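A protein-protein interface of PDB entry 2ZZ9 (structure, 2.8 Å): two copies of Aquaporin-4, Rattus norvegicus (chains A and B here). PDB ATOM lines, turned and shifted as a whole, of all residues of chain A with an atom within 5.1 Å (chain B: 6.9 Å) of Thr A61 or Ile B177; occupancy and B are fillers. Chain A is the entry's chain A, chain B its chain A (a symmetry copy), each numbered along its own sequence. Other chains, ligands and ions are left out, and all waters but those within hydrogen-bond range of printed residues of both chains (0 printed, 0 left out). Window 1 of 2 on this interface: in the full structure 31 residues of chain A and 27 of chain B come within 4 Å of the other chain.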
ATOM      1  N   LEU A  29       7.653  26.302  -8.668  1.00  0.00           N
ATOM      2  CA  LEU A  29       8.514  25.692  -7.643  1.00  0.00           C
ATOM      3  C   LEU A  29       9.332  24.542  -8.204  1.00  0.00           C
ATOM      4  O   LEU A  29      10.551  24.499  -8.028  1.00  0.00           O
ATOM      5  CB  LEU A  29       7.735  25.275  -6.376  1.00  0.00           C
ATOM      6  CG  LEU A  29       7.294  26.351  -5.350  1.00  0.00           C
ATOM      7  CD1 LEU A  29       8.420  26.813  -4.421  1.00  0.00           C
ATOM      8  CD2 LEU A  29       6.628  27.588  -6.007  1.00  0.00           C
ATOM      9  N   LEU A  53      12.213  14.561  -6.324  1.00  0.00           N
ATOM     10  CA  LEU A  53      11.478  14.849  -5.072  1.00  0.00           C
ATOM     11  C   LEU A  53      10.757  16.192  -5.144  1.00  0.00           C
ATOM     12  O   LEU A  53       9.682  16.366  -4.567  1.00  0.00           O
ATOM     13  CB  LEU A  53      12.388  14.901  -3.856  1.00  0.00           C
ATOM     14  CG  LEU A  53      12.966  13.656  -3.204  1.00  0.00           C
ATOM     15  CD1 LEU A  53      13.639  14.075  -1.911  1.00  0.00           C
ATOM     16  CD2 LEU A  53      11.939  12.544  -2.974  1.00  0.00           C
ATOM     17  N   CYS A  54      11.360  17.144  -5.847  1.00  0.00           N
ATOM     18  CA  CYS A  54      10.775  18.467  -5.934  1.00  0.00           C
ATOM     19  C   CYS A  54       9.397  18.362  -6.563  1.00  0.00           C
ATOM     20  O   CYS A  54       8.407  18.766  -5.963  1.00  0.00           O
ATOM     21  CB  CYS A  54      11.671  19.388  -6.753  1.00  0.00           C
ATOM     22  SG  CYS A  54      11.081  21.053  -6.740  1.00  0.00           S
ATOM     23  N   GLY A  56       7.426  15.845  -7.189  1.00  0.00           N
ATOM     24  CA  GLY A  56       6.452  14.941  -6.615  1.00  0.00           C
ATOM     25  C   GLY A  56       5.835  15.553  -5.374  1.00  0.00           C
ATOM     26  O   GLY A  56       4.606  15.617  -5.240  1.00  0.00           O
ATOM     27  N   LEU A  57       6.699  15.993  -4.463  1.00  0.00           N
ATOM     28  CA  LEU A  57       6.295  16.665  -3.243  1.00  0.00           C
ATOM     29  C   LEU A  57       5.551  17.977  -3.544  1.00  0.00           C
ATOM     30  O   LEU A  57       4.755  18.439  -2.722  1.00  0.00           O
ATOM     31  CB  LEU A  57       7.528  16.922  -2.357  1.00  0.00           C
ATOM     32  CG  LEU A  57       8.140  15.877  -1.397  1.00  0.00           C
ATOM     33  CD1 LEU A  57       9.029  14.855  -2.093  1.00  0.00           C
ATOM     34  CD2 LEU A  57       8.951  16.584  -0.325  1.00  0.00           C
ATOM     35  N   SER A  58       5.809  18.566  -4.716  1.00  0.00           N
ATOM     36  CA  SER A  58       5.183  19.845  -5.100  1.00  0.00           C
ATOM     37  C   SER A  58       3.730  19.605  -5.402  1.00  0.00           C
ATOM     38  O   SER A  58       2.867  20.393  -5.026  1.00  0.00           O
ATOM     39  CB  SER A  58       5.865  20.476  -6.332  1.00  0.00           C
ATOM     40  OG  SER A  58       7.121  21.033  -5.979  1.00  0.00           O
ATOM     41  N   ILE A  59       3.497  18.505  -6.117  1.00  0.00           N
ATOM     42  CA  ILE A  59       2.167  18.028  -6.468  1.00  0.00           C
ATOM     43  C   ILE A  59       1.433  17.519  -5.238  1.00  0.00           C
ATOM     44  O   ILE A  59       0.238  17.750  -5.083  1.00  0.00           O
ATOM     45  CB  ILE A  59       2.272  16.910  -7.499  1.00  0.00           C
ATOM     46  CG1 ILE A  59       2.559  17.502  -8.882  1.00  0.00           C
ATOM     47  CG2 ILE A  59       1.013  16.072  -7.519  1.00  0.00           C
ATOM     48  CD1 ILE A  59       1.366  18.219  -9.558  1.00  0.00           C
ATOM     49  N   ALA A  60       2.171  16.838  -4.370  1.00  0.00           N
ATOM     50  CA  ALA A  60       1.639  16.287  -3.146  1.00  0.00           C
ATOM     51  C   ALA A  60       1.215  17.430  -2.266  1.00  0.00           C
ATOM     52  O   ALA A  60       0.336  17.293  -1.409  1.00  0.00           O
ATOM     53  CB  ALA A  60       2.695  15.496  -2.446  1.00  0.00           C
ATOM     54  N   THR A  61       1.862  18.562  -2.463  1.00  0.00           N
ATOM     55  CA  THR A  61       1.592  19.717  -1.651  1.00  0.00           C
ATOM     56  C   THR A  61       0.368  20.411  -2.227  1.00  0.00           C
ATOM     57  O   THR A  61      -0.527  20.817  -1.492  1.00  0.00           O
ATOM     58  CB  THR A  61       2.839  20.617  -1.623  1.00  0.00           C
ATOM     59  OG1 THR A  61       3.880  19.940  -0.903  1.00  0.00           O
ATOM     60  CG2 THR A  61       2.569  21.948  -0.983  1.00  0.00           C
ATOM     61  N   MET A  62       0.325  20.510  -3.549  1.00  0.00           N
ATOM     62  CA  MET A  62      -0.706  21.273  -4.223  1.00  0.00           C
ATOM     63  C   MET A  62      -2.063  20.614  -4.077  1.00  0.00           C
ATOM     64  O   MET A  62      -3.072  21.293  -3.884  1.00  0.00           O
ATOM     65  CB  MET A  62      -0.362  21.514  -5.703  1.00  0.00           C
ATOM     66  CG  MET A  62       0.683  22.601  -5.956  1.00  0.00           C
ATOM     67  SD  MET A  62       0.847  23.858  -4.651  1.00  0.00           S
ATOM     68  CE  MET A  62      -0.130  25.189  -5.302  1.00  0.00           C
ATOM     69  N   VAL A  63      -2.089  19.293  -4.165  1.00  0.00           N
ATOM     70  CA  VAL A  63      -3.328  18.573  -3.945  1.00  0.00           C
ATOM     71  C   VAL A  63      -3.747  18.763  -2.483  1.00  0.00           C
ATOM     72  O   VAL A  63      -4.931  18.879  -2.175  1.00  0.00           O
ATOM     73  CB  VAL A  63      -3.194  17.086  -4.304  1.00  0.00           C
ATOM     74  CG1 VAL A  63      -2.820  16.913  -5.775  1.00  0.00           C
ATOM     75  CG2 VAL A  63      -2.151  16.453  -3.454  1.00  0.00           C
ATOM     76  N   GLN A  64      -2.774  18.823  -1.585  1.00  0.00           N
ATOM     77  CA  GLN A  64      -3.068  19.098  -0.192  1.00  0.00           C
ATOM     78  C   GLN A  64      -3.682  20.492   0.040  1.00  0.00           C
ATOM     79  O   GLN A  64      -4.498  20.651   0.943  1.00  0.00           O
ATOM     80  CB  GLN A  64      -1.822  18.867   0.686  1.00  0.00           C
ATOM     81  CG  GLN A  64      -1.969  17.742   1.738  1.00  0.00           C
ATOM     82  CD  GLN A  64      -2.509  18.254   3.086  1.00  0.00           C
ATOM     83  OE1 GLN A  64      -3.196  19.271   3.143  1.00  0.00           O
ATOM     84  NE2 GLN A  64      -2.194  17.545   4.168  1.00  0.00           N
ATOM     85  N   CYS A  65      -3.311  21.487  -0.767  1.00  0.00           N
ATOM     86  CA  CYS A  65      -3.810  22.868  -0.587  1.00  0.00           C
ATOM     87  C   CYS A  65      -5.157  23.109  -1.248  1.00  0.00           C
ATOM     88  O   CYS A  65      -5.927  23.970  -0.821  1.00  0.00           O
ATOM     89  CB  CYS A  65      -2.843  23.890  -1.195  1.00  0.00           C
ATOM     90  SG  CYS A  65      -1.198  23.892  -0.527  1.00  0.00           S
ATOM     91  N   SER B  52      17.700  20.530   2.262  1.00  0.00           N
ATOM     92  CA  SER B  52      16.266  20.537   2.016  1.00  0.00           C
ATOM     93  C   SER B  52      15.453  19.576   2.893  1.00  0.00           C
ATOM     94  O   SER B  52      14.521  20.027   3.556  1.00  0.00           O
ATOM     95  CB  SER B  52      16.004  20.291   0.530  1.00  0.00           C
ATOM     96  OG  SER B  52      16.544  21.364  -0.217  1.00  0.00           O
ATOM     97  N   ILE B 144       6.913  31.888  -1.602  1.00  0.00           N
ATOM     98  CA  ILE B 144       7.093  30.564  -1.025  1.00  0.00           C
ATOM     99  C   ILE B 144       6.474  30.516   0.347  1.00  0.00           C
ATOM    100  O   ILE B 144       5.762  29.567   0.683  1.00  0.00           O
ATOM    101  CB  ILE B 144       8.572  30.095  -0.970  1.00  0.00           C
ATOM    102  CG1 ILE B 144       9.457  31.115  -0.268  1.00  0.00           C
ATOM    103  CG2 ILE B 144       9.089  29.745  -2.363  1.00  0.00           C
ATOM    104  CD1 ILE B 144      10.763  30.556   0.172  1.00  0.00           C
ATOM    105  N   GLN B 147       2.843  29.722  -0.439  1.00  0.00           N
ATOM    106  CA  GLN B 147       2.755  28.283  -0.657  1.00  0.00           C
ATOM    107  C   GLN B 147       2.849  27.491   0.657  1.00  0.00           C
ATOM    108  O   GLN B 147       2.288  26.406   0.789  1.00  0.00           O
ATOM    109  CB  GLN B 147       3.863  27.884  -1.662  1.00  0.00           C
ATOM    110  CG  GLN B 147       4.323  26.432  -1.682  1.00  0.00           C
ATOM    111  CD  GLN B 147       5.316  26.121  -0.588  1.00  0.00           C
ATOM    112  OE1 GLN B 147       5.435  24.981  -0.145  1.00  0.00           O
ATOM    113  NE2 GLN B 147       6.022  27.137  -0.133  1.00  0.00           N
ATOM    114  N   LEU B 148       3.559  28.051   1.627  1.00  0.00           N
ATOM    115  CA  LEU B 148       3.848  27.341   2.852  1.00  0.00           C
ATOM    116  C   LEU B 148       2.787  27.611   3.903  1.00  0.00           C
ATOM    117  O   LEU B 148       2.367  26.696   4.624  1.00  0.00           O
ATOM    118  CB  LEU B 148       5.242  27.707   3.375  1.00  0.00           C
ATOM    119  CG  LEU B 148       5.473  27.451   4.867  1.00  0.00           C
ATOM    120  CD1 LEU B 148       5.737  25.968   5.142  1.00  0.00           C
ATOM    121  CD2 LEU B 148       6.575  28.326   5.415  1.00  0.00           C
ATOM    122  N   THR B 151      -0.383  25.880   2.826  1.00  0.00           N
ATOM    123  CA  THR B 151      -0.316  24.483   3.280  1.00  0.00           C
ATOM    124  C   THR B 151      -0.778  24.332   4.738  1.00  0.00           C
ATOM    125  O   THR B 151      -1.582  23.447   5.042  1.00  0.00           O
ATOM    126  CB  THR B 151       1.112  23.900   3.127  1.00  0.00           C
ATOM    127  OG1 THR B 151       1.489  23.918   1.743  1.00  0.00           O
ATOM    128  CG2 THR B 151       1.175  22.467   3.643  1.00  0.00           C
ATOM    129  N   SER B 155      -4.307  22.360   5.488  1.00  0.00           N
ATOM    130  CA  SER B 155      -4.136  21.136   6.277  1.00  0.00           C
ATOM    131  C   SER B 155      -4.664  21.267   7.709  1.00  0.00           C
ATOM    132  O   SER B 155      -5.125  20.286   8.292  1.00  0.00           O
ATOM    133  CB  SER B 155      -2.659  20.726   6.327  1.00  0.00           C
ATOM    134  OG  SER B 155      -2.049  20.810   5.053  1.00  0.00           O
ATOM    135  N   LEU B 169       3.827  16.134   8.346  1.00  0.00           N
ATOM    136  CA  LEU B 169       4.574  15.891   7.124  1.00  0.00           C
ATOM    137  C   LEU B 169       4.213  16.832   5.989  1.00  0.00           C
ATOM    138  O   LEU B 169       5.099  17.344   5.316  1.00  0.00           O
ATOM    139  CB  LEU B 169       4.469  14.441   6.676  1.00  0.00           C
ATOM    140  CG  LEU B 169       5.680  13.587   7.045  1.00  0.00           C
ATOM    141  CD1 LEU B 169       5.566  12.230   6.384  1.00  0.00           C
ATOM    142  CD2 LEU B 169       7.003  14.275   6.657  1.00  0.00           C
ATOM    143  N   ALA B 170       2.927  17.059   5.768  1.00  0.00           N
ATOM    144  CA  ALA B 170       2.506  18.041   4.781  1.00  0.00           C
ATOM    145  C   ALA B 170       3.264  19.360   4.994  1.00  0.00           C
ATOM    146  O   ALA B 170       3.994  19.824   4.118  1.00  0.00           O
ATOM    147  CB  ALA B 170       1.011  18.261   4.864  1.00  0.00           C
ATOM    148  N   GLY B 172       5.758  19.797   6.686  1.00  0.00           N
ATOM    149  CA  GLY B 172       7.183  19.528   6.527  1.00  0.00           C
ATOM    150  C   GLY B 172       7.517  19.668   5.060  1.00  0.00           C
ATOM    151  O   GLY B 172       8.304  20.528   4.673  1.00  0.00           O
ATOM    152  N   PHE B 173       6.870  18.837   4.247  1.00  0.00           N
ATOM    153  CA  PHE B 173       7.127  18.748   2.819  1.00  0.00           C
ATOM    154  C   PHE B 173       6.977  20.088   2.115  1.00  0.00           C
ATOM    155  O   PHE B 173       7.471  20.279   1.005  1.00  0.00           O
ATOM    156  CB  PHE B 173       6.196  17.711   2.186  1.00  0.00           C
ATOM    157  CG  PHE B 173       6.537  16.285   2.540  1.00  0.00           C
ATOM    158  CD1 PHE B 173       7.871  15.825   2.481  1.00  0.00           C
ATOM    159  CD2 PHE B 173       5.530  15.384   2.900  1.00  0.00           C
ATOM    160  CE1 PHE B 173       8.197  14.497   2.782  1.00  0.00           C
ATOM    161  CE2 PHE B 173       5.840  14.050   3.220  1.00  0.00           C
ATOM    162  CZ  PHE B 173       7.176  13.605   3.156  1.00  0.00           C
ATOM    163  N   SER B 174       6.283  21.015   2.768  1.00  0.00           N
ATOM    164  CA  SER B 174       6.037  22.330   2.186  1.00  0.00           C
ATOM    165  C   SER B 174       7.289  23.165   2.361  1.00  0.00           C
ATOM    166  O   SER B 174       7.771  23.803   1.421  1.00  0.00           O
ATOM    167  CB  SER B 174       4.852  22.993   2.861  1.00  0.00           C
ATOM    168  OG  SER B 174       4.492  24.148   2.151  1.00  0.00           O
ATOM    169  N   VAL B 175       7.812  23.139   3.580  1.00  0.00           N
ATOM    170  CA  VAL B 175       9.121  23.669   3.863  1.00  0.00           C
ATOM    171  C   VAL B 175      10.131  23.095   2.862  1.00  0.00           C
ATOM    172  O   VAL B 175      11.020  23.797   2.388  1.00  0.00           O
ATOM    173  CB  VAL B 175       9.544  23.320   5.307  1.00  0.00           C
ATOM    174  CG1 VAL B 175      10.908  23.954   5.660  1.00  0.00           C
ATOM    175  CG2 VAL B 175       8.491  23.780   6.294  1.00  0.00           C
ATOM    176  N   ALA B 176       9.962  21.817   2.544  1.00  0.00           N
ATOM    177  CA  ALA B 176      10.943  21.068   1.768  1.00  0.00           C
ATOM    178  C   ALA B 176      11.012  21.598   0.352  1.00  0.00           C
ATOM    179  O   ALA B 176      11.919  22.352   0.018  1.00  0.00           O
ATOM    180  CB  ALA B 176      10.625  19.594   1.775  1.00  0.00           C
ATOM    181  N   ILE B 177      10.052  21.203  -0.469  1.00  0.00           N
ATOM    182  CA  ILE B 177       9.907  21.742  -1.802  1.00  0.00           C
ATOM    183  C   ILE B 177      10.171  23.250  -1.855  1.00  0.00           C
ATOM    184  O   ILE B 177      10.547  23.786  -2.901  1.00  0.00           O
ATOM    185  CB  ILE B 177       8.499  21.446  -2.364  1.00  0.00           C
ATOM    186  CG1 ILE B 177       7.405  22.170  -1.569  1.00  0.00           C
ATOM    187  CG2 ILE B 177       8.237  19.934  -2.393  1.00  0.00           C
ATOM    188  CD1 ILE B 177       6.168  22.390  -2.358  1.00  0.00           C
ATOM    189  N   GLY B 178       9.964  23.930  -0.729  1.00  0.00           N
ATOM    190  CA  GLY B 178      10.231  25.368  -0.617  1.00  0.00           C
ATOM    191  C   GLY B 178      11.725  25.661  -0.622  1.00  0.00           C
ATOM    192  O   GLY B 178      12.176  26.604  -1.275  1.00  0.00           O
ATOM    193  N   HIS B 179      12.480  24.854   0.124  1.00  0.00           N
ATOM    194  CA  HIS B 179      13.942  24.864   0.090  1.00  0.00           C
ATOM    195  C   HIS B 179      14.431  24.268  -1.219  1.00  0.00           C
ATOM    196  O   HIS B 179      15.341  24.802  -1.851  1.00  0.00           O
ATOM    197  CB  HIS B 179      14.494  24.058   1.256  1.00  0.00           C
ATOM    198  CG  HIS B 179      14.476  24.804   2.546  1.00  0.00           C
ATOM    199  ND1 HIS B 179      13.375  24.829   3.376  1.00  0.00           N
ATOM    200  CD2 HIS B 179      15.414  25.579   3.136  1.00  0.00           C
ATOM    201  CE1 HIS B 179      13.639  25.583   4.428  1.00  0.00           C
ATOM    202  NE2 HIS B 179      14.869  26.049   4.308  1.00  0.00           N
ATOM    203  N   LEU B 180      13.798  23.169  -1.622  1.00  0.00           N
ATOM    204  CA  LEU B 180      14.077  22.496  -2.871  1.00  0.00           C
ATOM    205  C   LEU B 180      14.059  23.370  -4.134  1.00  0.00           C
ATOM    206  O   LEU B 180      14.265  22.849  -5.239  1.00  0.00           O
ATOM    207  CB  LEU B 180      13.110  21.328  -3.051  1.00  0.00           C
ATOM    208  CG  LEU B 180      13.575  19.976  -2.521  1.00  0.00           C
ATOM    209  CD1 LEU B 180      12.439  18.947  -2.618  1.00  0.00           C
ATOM    210  CD2 LEU B 180      14.847  19.517  -3.295  1.00  0.00           C
ATOM    211  N   PHE B 181      13.806  24.672  -3.987  1.00  0.00           N
ATOM    212  CA  PHE B 181      13.842  25.622  -5.116  1.00  0.00           C
ATOM    213  C   PHE B 181      14.626  26.903  -4.779  1.00  0.00           C
ATOM    214  O   PHE B 181      15.496  27.333  -5.545  1.00  0.00           O
ATOM    215  CB  PHE B 181      12.417  25.962  -5.615  1.00  0.00           C
ATOM    216  CG  PHE B 181      12.287  27.337  -6.239  1.00  0.00           C
ATOM    217  CD1 PHE B 181      12.825  27.616  -7.492  1.00  0.00           C
ATOM    218  CD2 PHE B 181      11.615  28.365  -5.571  1.00  0.00           C
ATOM    219  CE1 PHE B 181      12.691  28.898  -8.068  1.00  0.00           C
ATOM    220  CE2 PHE B 181      11.494  29.657  -6.143  1.00  0.00           C
ATOM    221  CZ  PHE B 181      12.036  29.916  -7.393  1.00  0.00           C
ATOM    222  N   ALA B 182      14.311  27.488  -3.627  1.00  0.00           N
ATOM    223  CA  ALA B 182      14.651  28.872  -3.354  1.00  0.00           C
ATOM    224  C   ALA B 182      16.044  29.008  -2.806  1.00  0.00           C
ATOM    225  O   ALA B 182      16.583  30.122  -2.757  1.00  0.00           O
ATOM    226  CB  ALA B 182      13.591  29.525  -2.378  1.00  0.00           C
ATOM    227  N   MET B 190      11.644  31.792   4.276  1.00  0.00           N
ATOM    228  CA  MET B 190      10.194  31.708   4.498  1.00  0.00           C
ATOM    229  C   MET B 190       9.813  31.747   5.995  1.00  0.00           C
ATOM    230  O   MET B 190       8.748  31.250   6.390  1.00  0.00           O
ATOM    231  CB  MET B 190       9.535  30.514   3.757  1.00  0.00           C
ATOM    232  CG  MET B 190      10.309  29.194   3.731  1.00  0.00           C
ATOM    233  SD  MET B 190       9.318  27.721   3.330  1.00  0.00           S
ATOM    234  CE  MET B 190       8.351  28.305   1.981  1.00  0.00           C
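OE1 of Gln A64 sits close to OG of Ser B155 (2.7 Å).
SG of Cys A65 sits close to OG1 of Thr B151 (3.5 Å).
Among the printed residues, pairs that only touch across the chains: Leu A29 with Ile B144, Leu A29 with Ile B177, Leu A29 with Phe B181, Cys A54 with Ile B177, Cys A54 with Leu B180, Leu A57 with Phe B173, Leu A57 with Ile B177, Ser A58 with Ile B177, Thr A61 with Thr B151, Thr A61 with Ile B177 and Gln A64 with Ala B170.
Of chain B, only Thr B151 and Ile B177 come within 4 Å of Thr A61.
Of the printed residues of chain B, Gln A64 touches Ser B155 and Ala B170.
Of the printed residues of chain A, Thr B151 touches Thr A61 and Cys A65.
Printed residues of chain A within 4 Å of Ile B177: Leu A29, Cys A54, Leu A57, Ser A58 and Thr A61.
The nearest residue of chain B that does not touch Thr A61 is Phe B173 (4.1 Å).
The nearest printed residue of chain A that does not touch Ile B177 is Leu A53 (4.4 Å).
The nearest printed residue of chain A that does not touch Leu B180 is Leu A53 (4.1 Å).
Hydrophobic or aromatic side chains of chain A within 4 Å of the printed part of chain B: Leu A29 and Leu A57.
Of the 20 printed residues of chain B, 8 touch a printed residue of chain A.
Hydrophobic or aromatic side chains of chain B within 4 Å of the printed part of chain A: Ile B144, Ala B170, Phe B173, Ile B177, Leu B180 and Phe B181.
Among the printed residues, no Asp or Glu carboxylate lies within 4 Å of a Lys or Arg side-chain nitrogen of the other chain.
No position is printed for both chains.
Of the 13 pairs that touch across the chains among the printed residues, none has its exchanged pair printed and touching as well.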
